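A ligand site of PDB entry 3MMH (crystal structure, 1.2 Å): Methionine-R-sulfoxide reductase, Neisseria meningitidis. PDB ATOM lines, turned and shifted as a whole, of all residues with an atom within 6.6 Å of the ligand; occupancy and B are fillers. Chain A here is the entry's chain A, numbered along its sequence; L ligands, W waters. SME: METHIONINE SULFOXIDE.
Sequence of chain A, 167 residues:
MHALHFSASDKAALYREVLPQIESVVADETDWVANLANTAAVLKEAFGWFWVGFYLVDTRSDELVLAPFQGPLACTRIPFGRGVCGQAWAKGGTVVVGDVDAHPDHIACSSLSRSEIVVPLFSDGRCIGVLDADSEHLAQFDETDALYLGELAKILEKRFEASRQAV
S of the ligand lies close to SG of Cys 109 (3.6 Å). The side-chain carboxylate of Asp 132 lies close to a sulfur (S) of the ligand, 3.7 Å away. OE of the ligand sits close to OD1 of Asp 134 (3.4 Å). Trp 51 touches the ligand (CE2 to CE, 3.5 Å). Tyr 55 touches the ligand (OH to CG, 3.6 Å). CD1 of Ile 78 touches CB of the ligand (3.7 Å). Gly 83 touches the ligand. Hydrophobic or aromatic side chains within 4 Å of the ligand: Trp 51, Tyr 55, Ile 78, Val 84, His 106 and Ile 107. Of the 27 residues printed, 12 come within 4 Å of the ligand. Along chain A the residues within 4 Å of the ligand span positions 51 to 134.
The side-chain sulfur (SG) of Cys 75 is disulfide-bonded to the side-chain sulfur (SG) of Cys 109, at 2.1 Å. NE2 of His 106 lies close to OE1 of Glu 116 (3.3 Å). The side-chain hydroxyl (OH) of Tyr 55 is in hydrogen-bond range of the backbone carbonyl oxygen (O) of Cys 75 (2.8 Å). The backbone NH (N) of Asp 134 lies within hydrogen-bond range of the backbone carbonyl oxygen (O) of Trp 51, 2.8 Å away. The side-chain carboxylate of Asp 132 lies close to the side-chain carboxylate of Glu 116, at 2.5 Å. N of Gly 83 lies within hydrogen-bond range of OD2 of Asp 105, 3.1 Å away. The backbone carbonyl oxygen (O) of Pro 72 sits at hydrogen-bond distance from the indole nitrogen (NE1) of Trp 51.
Water W2 lies within hydrogen-bond range of OE of the ligand (2.7 Å), N of Ser 110 (3.0 Å), N of Cys 109 (3.1 Å) and OG of Ser 113 (3.1 Å).
The backbone NH of Cys 85 sits at hydrogen-bond distance from an oxygen (O) of the ligand, 2.8 Å away. The side-chain carboxylate (OE1) of Glu 116 lies within salt-bridge range of a nitrogen (N) of the ligand, at 2.9 Å. N of Val 84 lies within hydrogen-bond range of OXT of the ligand (2.8 Å). N of the ligand is in hydrogen-bond range of O of Ile 107, at 2.8 Å. The side-chain sulfur of Cys 85 lies close to an oxygen (O) of the ligand (3.5 Å). The backbone NH (N) of Ile 107 is in hydrogen-bond range of an oxygen (OXT) of the ligand. NE2 of His 106 sits at hydrogen-bond distance from N of the ligand, at 3.4 Å.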
ATOM      1  N   TRP A  51     -21.153 -17.083  -4.047  1.00  0.00           N
ATOM      2  CA  TRP A  51     -20.858 -18.461  -4.150  1.00  0.00           C
ATOM      3  C   TRP A  51     -21.728 -19.201  -3.204  1.00  0.00           C
ATOM      4  O   TRP A  51     -21.884 -18.800  -2.040  1.00  0.00           O
ATOM      5  CB  TRP A  51     -19.358 -18.699  -3.825  1.00  0.00           C
ATOM      6  CG  TRP A  51     -18.734 -19.982  -4.291  1.00  0.00           C
ATOM      7  CD1 TRP A  51     -17.998 -20.116  -5.440  1.00  0.00           C
ATOM      8  CD2 TRP A  51     -18.807 -21.296  -3.683  1.00  0.00           C
ATOM      9  NE1 TRP A  51     -17.593 -21.404  -5.535  1.00  0.00           N
ATOM     10  CE2 TRP A  51     -18.052 -22.156  -4.491  1.00  0.00           C
ATOM     11  CE3 TRP A  51     -19.356 -21.808  -2.515  1.00  0.00           C
ATOM     12  CZ2 TRP A  51     -17.866 -23.490  -4.207  1.00  0.00           C
ATOM     13  CZ3 TRP A  51     -19.220 -23.123  -2.210  1.00  0.00           C
ATOM     14  CH2 TRP A  51     -18.485 -23.969  -3.056  1.00  0.00           C
ATOM     15  N   TYR A  55     -19.225 -28.994   0.030  1.00  0.00           N
ATOM     16  CA  TYR A  55     -18.078 -29.906   0.060  1.00  0.00           C
ATOM     17  C   TYR A  55     -18.480 -31.133   0.828  1.00  0.00           C
ATOM     18  O   TYR A  55     -19.257 -31.033   1.803  1.00  0.00           O
ATOM     19  CB  TYR A  55     -16.854 -29.273   0.751  1.00  0.00           C
ATOM     20  CG  TYR A  55     -16.152 -28.190   0.009  1.00  0.00           C
ATOM     21  CD1 TYR A  55     -14.914 -28.447  -0.611  1.00  0.00           C
ATOM     22  CD2 TYR A  55     -16.647 -26.864  -0.073  1.00  0.00           C
ATOM     23  CE1 TYR A  55     -14.273 -27.489  -1.304  1.00  0.00           C
ATOM     24  CE2 TYR A  55     -15.996 -25.875  -0.774  1.00  0.00           C
ATOM     25  CZ  TYR A  55     -14.789 -26.189  -1.429  1.00  0.00           C
ATOM     26  OH  TYR A  55     -14.147 -25.218  -2.151  1.00  0.00           O
ATOM     27  N   LEU A  66     -14.829 -30.782  -3.085  1.00  0.00           N
ATOM     28  CA  LEU A  66     -15.788 -29.963  -3.728  1.00  0.00           C
ATOM     29  C   LEU A  66     -16.873 -30.780  -4.386  1.00  0.00           C
ATOM     30  O   LEU A  66     -16.598 -31.749  -5.083  1.00  0.00           O
ATOM     31  CB  LEU A  66     -15.088 -29.091  -4.781  1.00  0.00           C
ATOM     32  CG  LEU A  66     -15.926 -28.040  -5.542  1.00  0.00           C
ATOM     33  CD1 LEU A  66     -16.510 -27.035  -4.581  1.00  0.00           C
ATOM     34  CD2 LEU A  66     -14.917 -27.422  -6.580  1.00  0.00           C
ATOM     35  N   PRO A  72     -18.022 -18.752  -8.976  1.00  0.00           N
ATOM     36  CA  PRO A  72     -16.745 -18.994  -9.645  1.00  0.00           C
ATOM     37  C   PRO A  72     -16.028 -20.260  -9.156  1.00  0.00           C
ATOM     38  O   PRO A  72     -16.277 -20.736  -8.056  1.00  0.00           O
ATOM     39  CB  PRO A  72     -15.960 -17.706  -9.383  1.00  0.00           C
ATOM     40  CG  PRO A  72     -16.544 -17.215  -8.089  1.00  0.00           C
ATOM     41  CD  PRO A  72     -18.016 -17.511  -8.194  1.00  0.00           C
ATOM     42  N   LEU A  73     -14.921 -20.562  -9.820  1.00  0.00           N
ATOM     43  CA  LEU A  73     -14.346 -21.969  -9.625  1.00  0.00           C
ATOM     44  C   LEU A  73     -13.751 -21.782  -8.242  1.00  0.00           C
ATOM     45  O   LEU A  73     -13.476 -20.687  -7.736  1.00  0.00           O
ATOM     46  CB  LEU A  73     -13.279 -22.275 -10.671  1.00  0.00           C
ATOM     47  CG  LEU A  73     -12.056 -21.367 -10.648  1.00  0.00           C
ATOM     48  CD1 LEU A  73     -11.015 -21.887  -9.675  1.00  0.00           C
ATOM     49  CD2 LEU A  73     -11.459 -21.226 -12.042  1.00  0.00           C
ATOM     50  N   ALA A  74     -13.544 -22.927  -7.629  1.00  0.00           N
ATOM     51  CA  ALA A  74     -13.170 -23.051  -6.246  1.00  0.00           C
ATOM     52  C   ALA A  74     -12.113 -24.081  -6.025  1.00  0.00           C
ATOM     53  O   ALA A  74     -11.839 -24.945  -6.872  1.00  0.00           O
ATOM     54  CB  ALA A  74     -14.419 -23.405  -5.332  1.00  0.00           C
ATOM     55  N   CYS A  75     -11.470 -24.033  -4.877  1.00  0.00           N
ATOM     56  CA  CYS A  75     -10.552 -25.070  -4.366  1.00  0.00           C
ATOM     57  C   CYS A  75     -11.217 -26.386  -4.340  1.00  0.00           C
ATOM     58  O   CYS A  75     -12.346 -26.467  -3.863  1.00  0.00           O
ATOM     59  CB  CYS A  75     -10.077 -24.778  -2.922  1.00  0.00           C
ATOM     60  SG  CYS A  75      -9.401 -23.091  -2.622  1.00  0.00           S
ATOM     61  N   ILE A  78     -10.193 -29.203   0.903  1.00  0.00           N
ATOM     62  CA  ILE A  78      -9.947 -28.439   2.151  1.00  0.00           C
ATOM     63  C   ILE A  78      -9.628 -29.471   3.257  1.00  0.00           C
ATOM     64  O   ILE A  78     -10.460 -30.284   3.603  1.00  0.00           O
ATOM     65  CB  ILE A  78     -11.163 -27.556   2.520  1.00  0.00           C
ATOM     66  CG1 ILE A  78     -11.462 -26.533   1.393  1.00  0.00           C
ATOM     67  CG2 ILE A  78     -10.857 -26.777   3.809  1.00  0.00           C
ATOM     68  CD1 ILE A  78     -12.729 -25.814   1.595  1.00  0.00           C
ATOM     69  N   ARG A  82      -8.864 -26.869   8.568  1.00  0.00           N
ATOM     70  CA  ARG A  82      -8.322 -25.691   7.896  1.00  0.00           C
ATOM     71  C   ARG A  82      -9.481 -24.932   7.248  1.00  0.00           C
ATOM     72  O   ARG A  82     -10.434 -25.539   6.710  1.00  0.00           O
ATOM     73  CB  ARG A  82      -7.366 -26.175   6.822  1.00  0.00           C
ATOM     74  CG  ARG A  82      -6.107 -26.914   7.361  1.00  0.00           C
ATOM     75  CD  ARG A  82      -5.222 -26.080   8.263  1.00  0.00           C
ATOM     76  NE  ARG A  82      -4.949 -24.735   7.738  1.00  0.00           N
ATOM     77  CZ  ARG A  82      -3.880 -24.468   7.008  1.00  0.00           C
ATOM     78  NH1 ARG A  82      -3.054 -25.371   6.648  1.00  0.00           N
ATOM     79  NH2 ARG A  82      -3.666 -23.233   6.583  1.00  0.00           N
ATOM     80  N   GLY A  83      -9.366 -23.613   7.213  1.00  0.00           N
ATOM     81  CA  GLY A  83     -10.375 -22.770   6.634  1.00  0.00           C
ATOM     82  C   GLY A  83     -11.632 -22.706   7.487  1.00  0.00           C
ATOM     83  O   GLY A  83     -11.792 -23.438   8.421  1.00  0.00           O
ATOM     84  N   VAL A  84     -12.560 -21.810   7.082  1.00  0.00           N
ATOM     85  CA  VAL A  84     -13.868 -21.808   7.739  1.00  0.00           C
ATOM     86  C   VAL A  84     -14.514 -23.218   7.595  1.00  0.00           C
ATOM     87  O   VAL A  84     -15.183 -23.673   8.497  1.00  0.00           O
ATOM     88  CB  VAL A  84     -14.736 -20.684   7.165  1.00  0.00           C
ATOM     89  CG1 VAL A  84     -16.033 -20.551   7.925  1.00  0.00           C
ATOM     90  CG2 VAL A  84     -13.991 -19.341   7.162  1.00  0.00           C
ATOM     91  N   CYS A  85     -14.399 -23.807   6.403  1.00  0.00           N
ATOM     92  CA  CYS A  85     -15.034 -25.087   6.161  1.00  0.00           C
ATOM     93  C   CYS A  85     -14.466 -26.211   7.067  1.00  0.00           C
ATOM     94  O   CYS A  85     -15.227 -26.938   7.662  1.00  0.00           O
ATOM     95  CB  CYS A  85     -14.929 -25.483   4.727  1.00  0.00           C
ATOM     96  SG  CYS A  85     -15.959 -24.524   3.565  1.00  0.00           S
ATOM     97  N   GLY A  86     -13.126 -26.282   7.127  1.00  0.00           N
ATOM     98  CA  GLY A  86     -12.527 -27.280   7.974  1.00  0.00           C
ATOM     99  C   GLY A  86     -12.732 -27.038   9.434  1.00  0.00           C
ATOM    100  O   GLY A  86     -12.764 -28.000  10.256  1.00  0.00           O
ATOM    101  N   GLN A  87     -12.817 -25.760   9.838  1.00  0.00           N
ATOM    102  CA  GLN A  87     -13.202 -25.397  11.200  1.00  0.00           C
ATOM    103  C   GLN A  87     -14.602 -25.789  11.578  1.00  0.00           C
ATOM    104  O   GLN A  87     -14.841 -26.297  12.695  1.00  0.00           O
ATOM    105  CB  GLN A  87     -13.066 -23.915  11.453  1.00  0.00           C
ATOM    106  CG  GLN A  87     -11.644 -23.417  11.447  1.00  0.00           C
ATOM    107  CD  GLN A  87     -11.499 -21.913  11.259  1.00  0.00           C
ATOM    108  OE1 GLN A  87     -12.476 -21.166  11.263  1.00  0.00           O
ATOM    109  NE2 GLN A  87     -10.268 -21.497  11.065  1.00  0.00           N
ATOM    110  N   VAL A 100     -13.987 -11.877   6.331  1.00  0.00           N
ATOM    111  CA  VAL A 100     -13.031 -12.947   6.135  1.00  0.00           C
ATOM    112  C   VAL A 100     -11.598 -12.514   6.485  1.00  0.00           C
ATOM    113  O   VAL A 100     -10.770 -13.327   6.867  1.00  0.00           O
ATOM    114  CB  VAL A 100     -13.107 -13.631   4.784  1.00  0.00           C
ATOM    115  CG1 VAL A 100     -14.500 -14.250   4.587  1.00  0.00           C
ATOM    116  CG2 VAL A 100     -12.627 -12.704   3.686  1.00  0.00           C
ATOM    117  N   HIS A 103     -10.871 -13.229  10.242  1.00  0.00           N
ATOM    118  CA  HIS A 103     -11.135 -14.581  10.635  1.00  0.00           C
ATOM    119  C   HIS A 103      -9.888 -15.406  10.594  1.00  0.00           C
ATOM    120  O   HIS A 103      -9.231 -15.458   9.542  1.00  0.00           O
ATOM    121  CB  HIS A 103     -12.219 -15.239   9.781  1.00  0.00           C
ATOM    122  CG  HIS A 103     -12.792 -16.407  10.464  1.00  0.00           C
ATOM    123  ND1 HIS A 103     -13.759 -16.318  11.459  1.00  0.00           N
ATOM    124  CD2 HIS A 103     -12.647 -17.727  10.187  1.00  0.00           C
ATOM    125  CE1 HIS A 103     -14.082 -17.557  11.824  1.00  0.00           C
ATOM    126  NE2 HIS A 103     -13.417 -18.412  11.077  1.00  0.00           N
ATOM    127  N   ASP A 105      -7.359 -18.062   9.700  1.00  0.00           N
ATOM    128  CA  ASP A 105      -7.136 -19.156   8.731  1.00  0.00           C
ATOM    129  C   ASP A 105      -8.260 -19.350   7.660  1.00  0.00           C
ATOM    130  O   ASP A 105      -8.445 -20.439   7.184  1.00  0.00           O
ATOM    131  CB  ASP A 105      -6.899 -20.491   9.446  1.00  0.00           C
ATOM    132  CG  ASP A 105      -6.335 -21.594   8.565  1.00  0.00           C
ATOM    133  OD1 ASP A 105      -5.426 -21.297   7.738  1.00  0.00           O
ATOM    134  OD2 ASP A 105      -6.769 -22.766   8.655  1.00  0.00           O
ATOM    135  N   HIS A 106      -8.947 -18.286   7.271  1.00  0.00           N
ATOM    136  CA  HIS A 106      -9.840 -18.292   6.117  1.00  0.00           C
ATOM    137  C   HIS A 106      -9.045 -18.729   4.878  1.00  0.00           C
ATOM    138  O   HIS A 106      -7.894 -18.280   4.657  1.00  0.00           O
ATOM    139  CB  HIS A 106     -10.445 -16.888   5.952  1.00  0.00           C
ATOM    140  CG  HIS A 106     -11.248 -16.727   4.724  1.00  0.00           C
ATOM    141  ND1 HIS A 106     -10.759 -16.089   3.608  1.00  0.00           N
ATOM    142  CD2 HIS A 106     -12.491 -17.161   4.384  1.00  0.00           C
ATOM    143  CE1 HIS A 106     -11.671 -16.095   2.656  1.00  0.00           C
ATOM    144  NE2 HIS A 106     -12.723 -16.775   3.085  1.00  0.00           N
ATOM    145  N   ILE A 107      -9.690 -19.584   4.084  1.00  0.00           N
ATOM    146  CA  ILE A 107      -9.105 -19.989   2.829  1.00  0.00           C
ATOM    147  C   ILE A 107      -9.805 -19.157   1.725  1.00  0.00           C
ATOM    148  O   ILE A 107     -11.016 -19.338   1.459  1.00  0.00           O
ATOM    149  CB  ILE A 107      -9.201 -21.496   2.624  1.00  0.00           C
ATOM    150  CG1 ILE A 107      -8.481 -22.283   3.682  1.00  0.00           C
ATOM    151  CG2 ILE A 107      -8.776 -21.862   1.192  1.00  0.00           C
ATOM    152  CD1 ILE A 107      -8.756 -23.760   3.591  1.00  0.00           C
ATOM    153  N   ALA A 108      -9.014 -18.350   1.027  1.00  0.00           N
ATOM    154  CA  ALA A 108      -9.513 -17.466   0.008  1.00  0.00           C
ATOM    155  C   ALA A 108      -9.480 -18.115  -1.401  1.00  0.00           C
ATOM    156  O   ALA A 108      -8.660 -17.747  -2.231  1.00  0.00           O
ATOM    157  CB  ALA A 108      -8.788 -16.047   0.052  1.00  0.00           C
ATOM    158  N   CYS A 109     -10.414 -19.002  -1.755  1.00  0.00           N
ATOM    159  CA  CYS A 109     -10.420 -19.635  -3.112  1.00  0.00           C
ATOM    160  C   CYS A 109     -10.719 -18.571  -4.134  1.00  0.00           C
ATOM    161  O   CYS A 109     -10.312 -18.705  -5.273  1.00  0.00           O
ATOM    162  CB  CYS A 109     -11.394 -20.844  -3.245  1.00  0.00           C
ATOM    163  SG  CYS A 109     -11.155 -22.071  -1.987  1.00  0.00           S
ATOM    164  N   SER A 110     -11.494 -17.560  -3.754  1.00  0.00           N
ATOM    165  CA  SER A 110     -11.582 -16.339  -4.541  1.00  0.00           C
ATOM    166  C   SER A 110     -11.105 -15.201  -3.750  1.00  0.00           C
ATOM    167  O   SER A 110     -11.442 -15.093  -2.563  1.00  0.00           O
ATOM    168  CB  SER A 110     -13.022 -16.103  -4.957  1.00  0.00           C
ATOM    169  OG  SER A 110     -13.189 -14.842  -5.529  1.00  0.00           O
ATOM    170  N   SER A 113     -14.362 -12.719  -2.158  1.00  0.00           N
ATOM    171  CA  SER A 113     -15.300 -12.912  -1.059  1.00  0.00           C
ATOM    172  C   SER A 113     -14.854 -12.160   0.198  1.00  0.00           C
ATOM    173  O   SER A 113     -13.673 -12.109   0.561  1.00  0.00           O
ATOM    174  CB  SER A 113     -15.545 -14.391  -0.808  1.00  0.00           C
ATOM    175  OG  SER A 113     -14.316 -14.981  -0.577  1.00  0.00           O
ATOM    176  N   GLU A 116     -18.842 -14.983   4.869  1.00  0.00           N
ATOM    177  CA  GLU A 116     -19.097 -16.396   4.633  1.00  0.00           C
ATOM    178  C   GLU A 116     -19.916 -17.003   5.752  1.00  0.00           C
ATOM    179  O   GLU A 116     -19.862 -16.543   6.922  1.00  0.00           O
ATOM    180  CB  GLU A 116     -17.730 -17.097   4.553  1.00  0.00           C
ATOM    181  CG  GLU A 116     -17.706 -18.578   4.280  1.00  0.00           C
ATOM    182  CD  GLU A 116     -16.389 -19.145   3.961  1.00  0.00           C
ATOM    183  OE1 GLU A 116     -15.356 -18.522   4.129  1.00  0.00           O
ATOM    184  OE2 GLU A 116     -16.294 -20.365   3.583  1.00  0.00           O
ATOM    185  N   VAL A 118     -20.668 -21.267   6.983  1.00  0.00           N
ATOM    186  CA  VAL A 118     -20.544 -22.694   6.775  1.00  0.00           C
ATOM    187  C   VAL A 118     -21.444 -23.435   7.731  1.00  0.00           C
ATOM    188  O   VAL A 118     -21.330 -23.220   8.937  1.00  0.00           O
ATOM    189  CB  VAL A 118     -19.095 -23.164   6.898  1.00  0.00           C
ATOM    190  CG1 VAL A 118     -19.021 -24.688   6.661  1.00  0.00           C
ATOM    191  CG2 VAL A 118     -18.195 -22.391   5.925  1.00  0.00           C
ATOM    192  N   ASP A 132     -21.522 -24.280   2.185  1.00  0.00           N
ATOM    193  CA  ASP A 132     -20.747 -23.056   2.281  1.00  0.00           C
ATOM    194  C   ASP A 132     -21.376 -21.993   1.379  1.00  0.00           C
ATOM    195  O   ASP A 132     -21.710 -22.272   0.218  1.00  0.00           O
ATOM    196  CB  ASP A 132     -19.300 -23.315   1.780  1.00  0.00           C
ATOM    197  CG  ASP A 132     -18.455 -22.099   1.845  1.00  0.00           C
ATOM    198  OD1 ASP A 132     -18.420 -21.463   2.860  1.00  0.00           O
ATOM    199  OD2 ASP A 132     -17.697 -21.842   0.913  1.00  0.00           O
ATOM    200  N   ASP A 134     -20.814 -17.702   0.303  1.00  0.00           N
ATOM    201  CA  ASP A 134     -19.870 -16.605   0.346  1.00  0.00           C
ATOM    202  C   ASP A 134     -20.487 -15.381  -0.349  1.00  0.00           C
ATOM    203  O   ASP A 134     -21.290 -15.512  -1.254  1.00  0.00           O
ATOM    204  CB  ASP A 134     -18.493 -17.013  -0.279  1.00  0.00           C
ATOM    205  CG  ASP A 134     -17.915 -18.249   0.334  1.00  0.00           C
ATOM    206  OD1 ASP A 134     -17.112 -18.101   1.271  1.00  0.00           O
ATOM    207  OD2 ASP A 134     -18.311 -19.368  -0.134  1.00  0.00           O
HETATM  208  N   SME L   1     -13.616 -19.910   2.294  1.00  0.00           N
HETATM  209  CA  SME L   1     -13.641 -21.369   2.526  1.00  0.00           C
HETATM  210  CB  SME L   1     -13.127 -22.179   1.312  1.00  0.00           C
HETATM  211  CG  SME L   1     -14.181 -22.494   0.240  1.00  0.00           C
HETATM  212  S   SME L   1     -14.489 -21.155  -0.827  1.00  0.00           S
HETATM  213  OE  SME L   1     -14.623 -19.808  -0.305  1.00  0.00           O
HETATM  214  CE  SME L   1     -15.754 -21.829  -1.813  1.00  0.00           C
HETATM  215  C   SME L   1     -12.899 -21.714   3.787  1.00  0.00           C
HETATM  216  O   SME L   1     -12.912 -22.895   4.166  1.00  0.00           O
HETATM  217  OXT SME L   1     -12.303 -20.775   4.449  1.00  0.00           O
HETATM  218  O   HOH W   1     -14.598 -16.982   1.241  1.00  0.00           O
HETATM  219  O   HOH W   2     -13.208 -17.787  -1.320  1.00  0.00           O
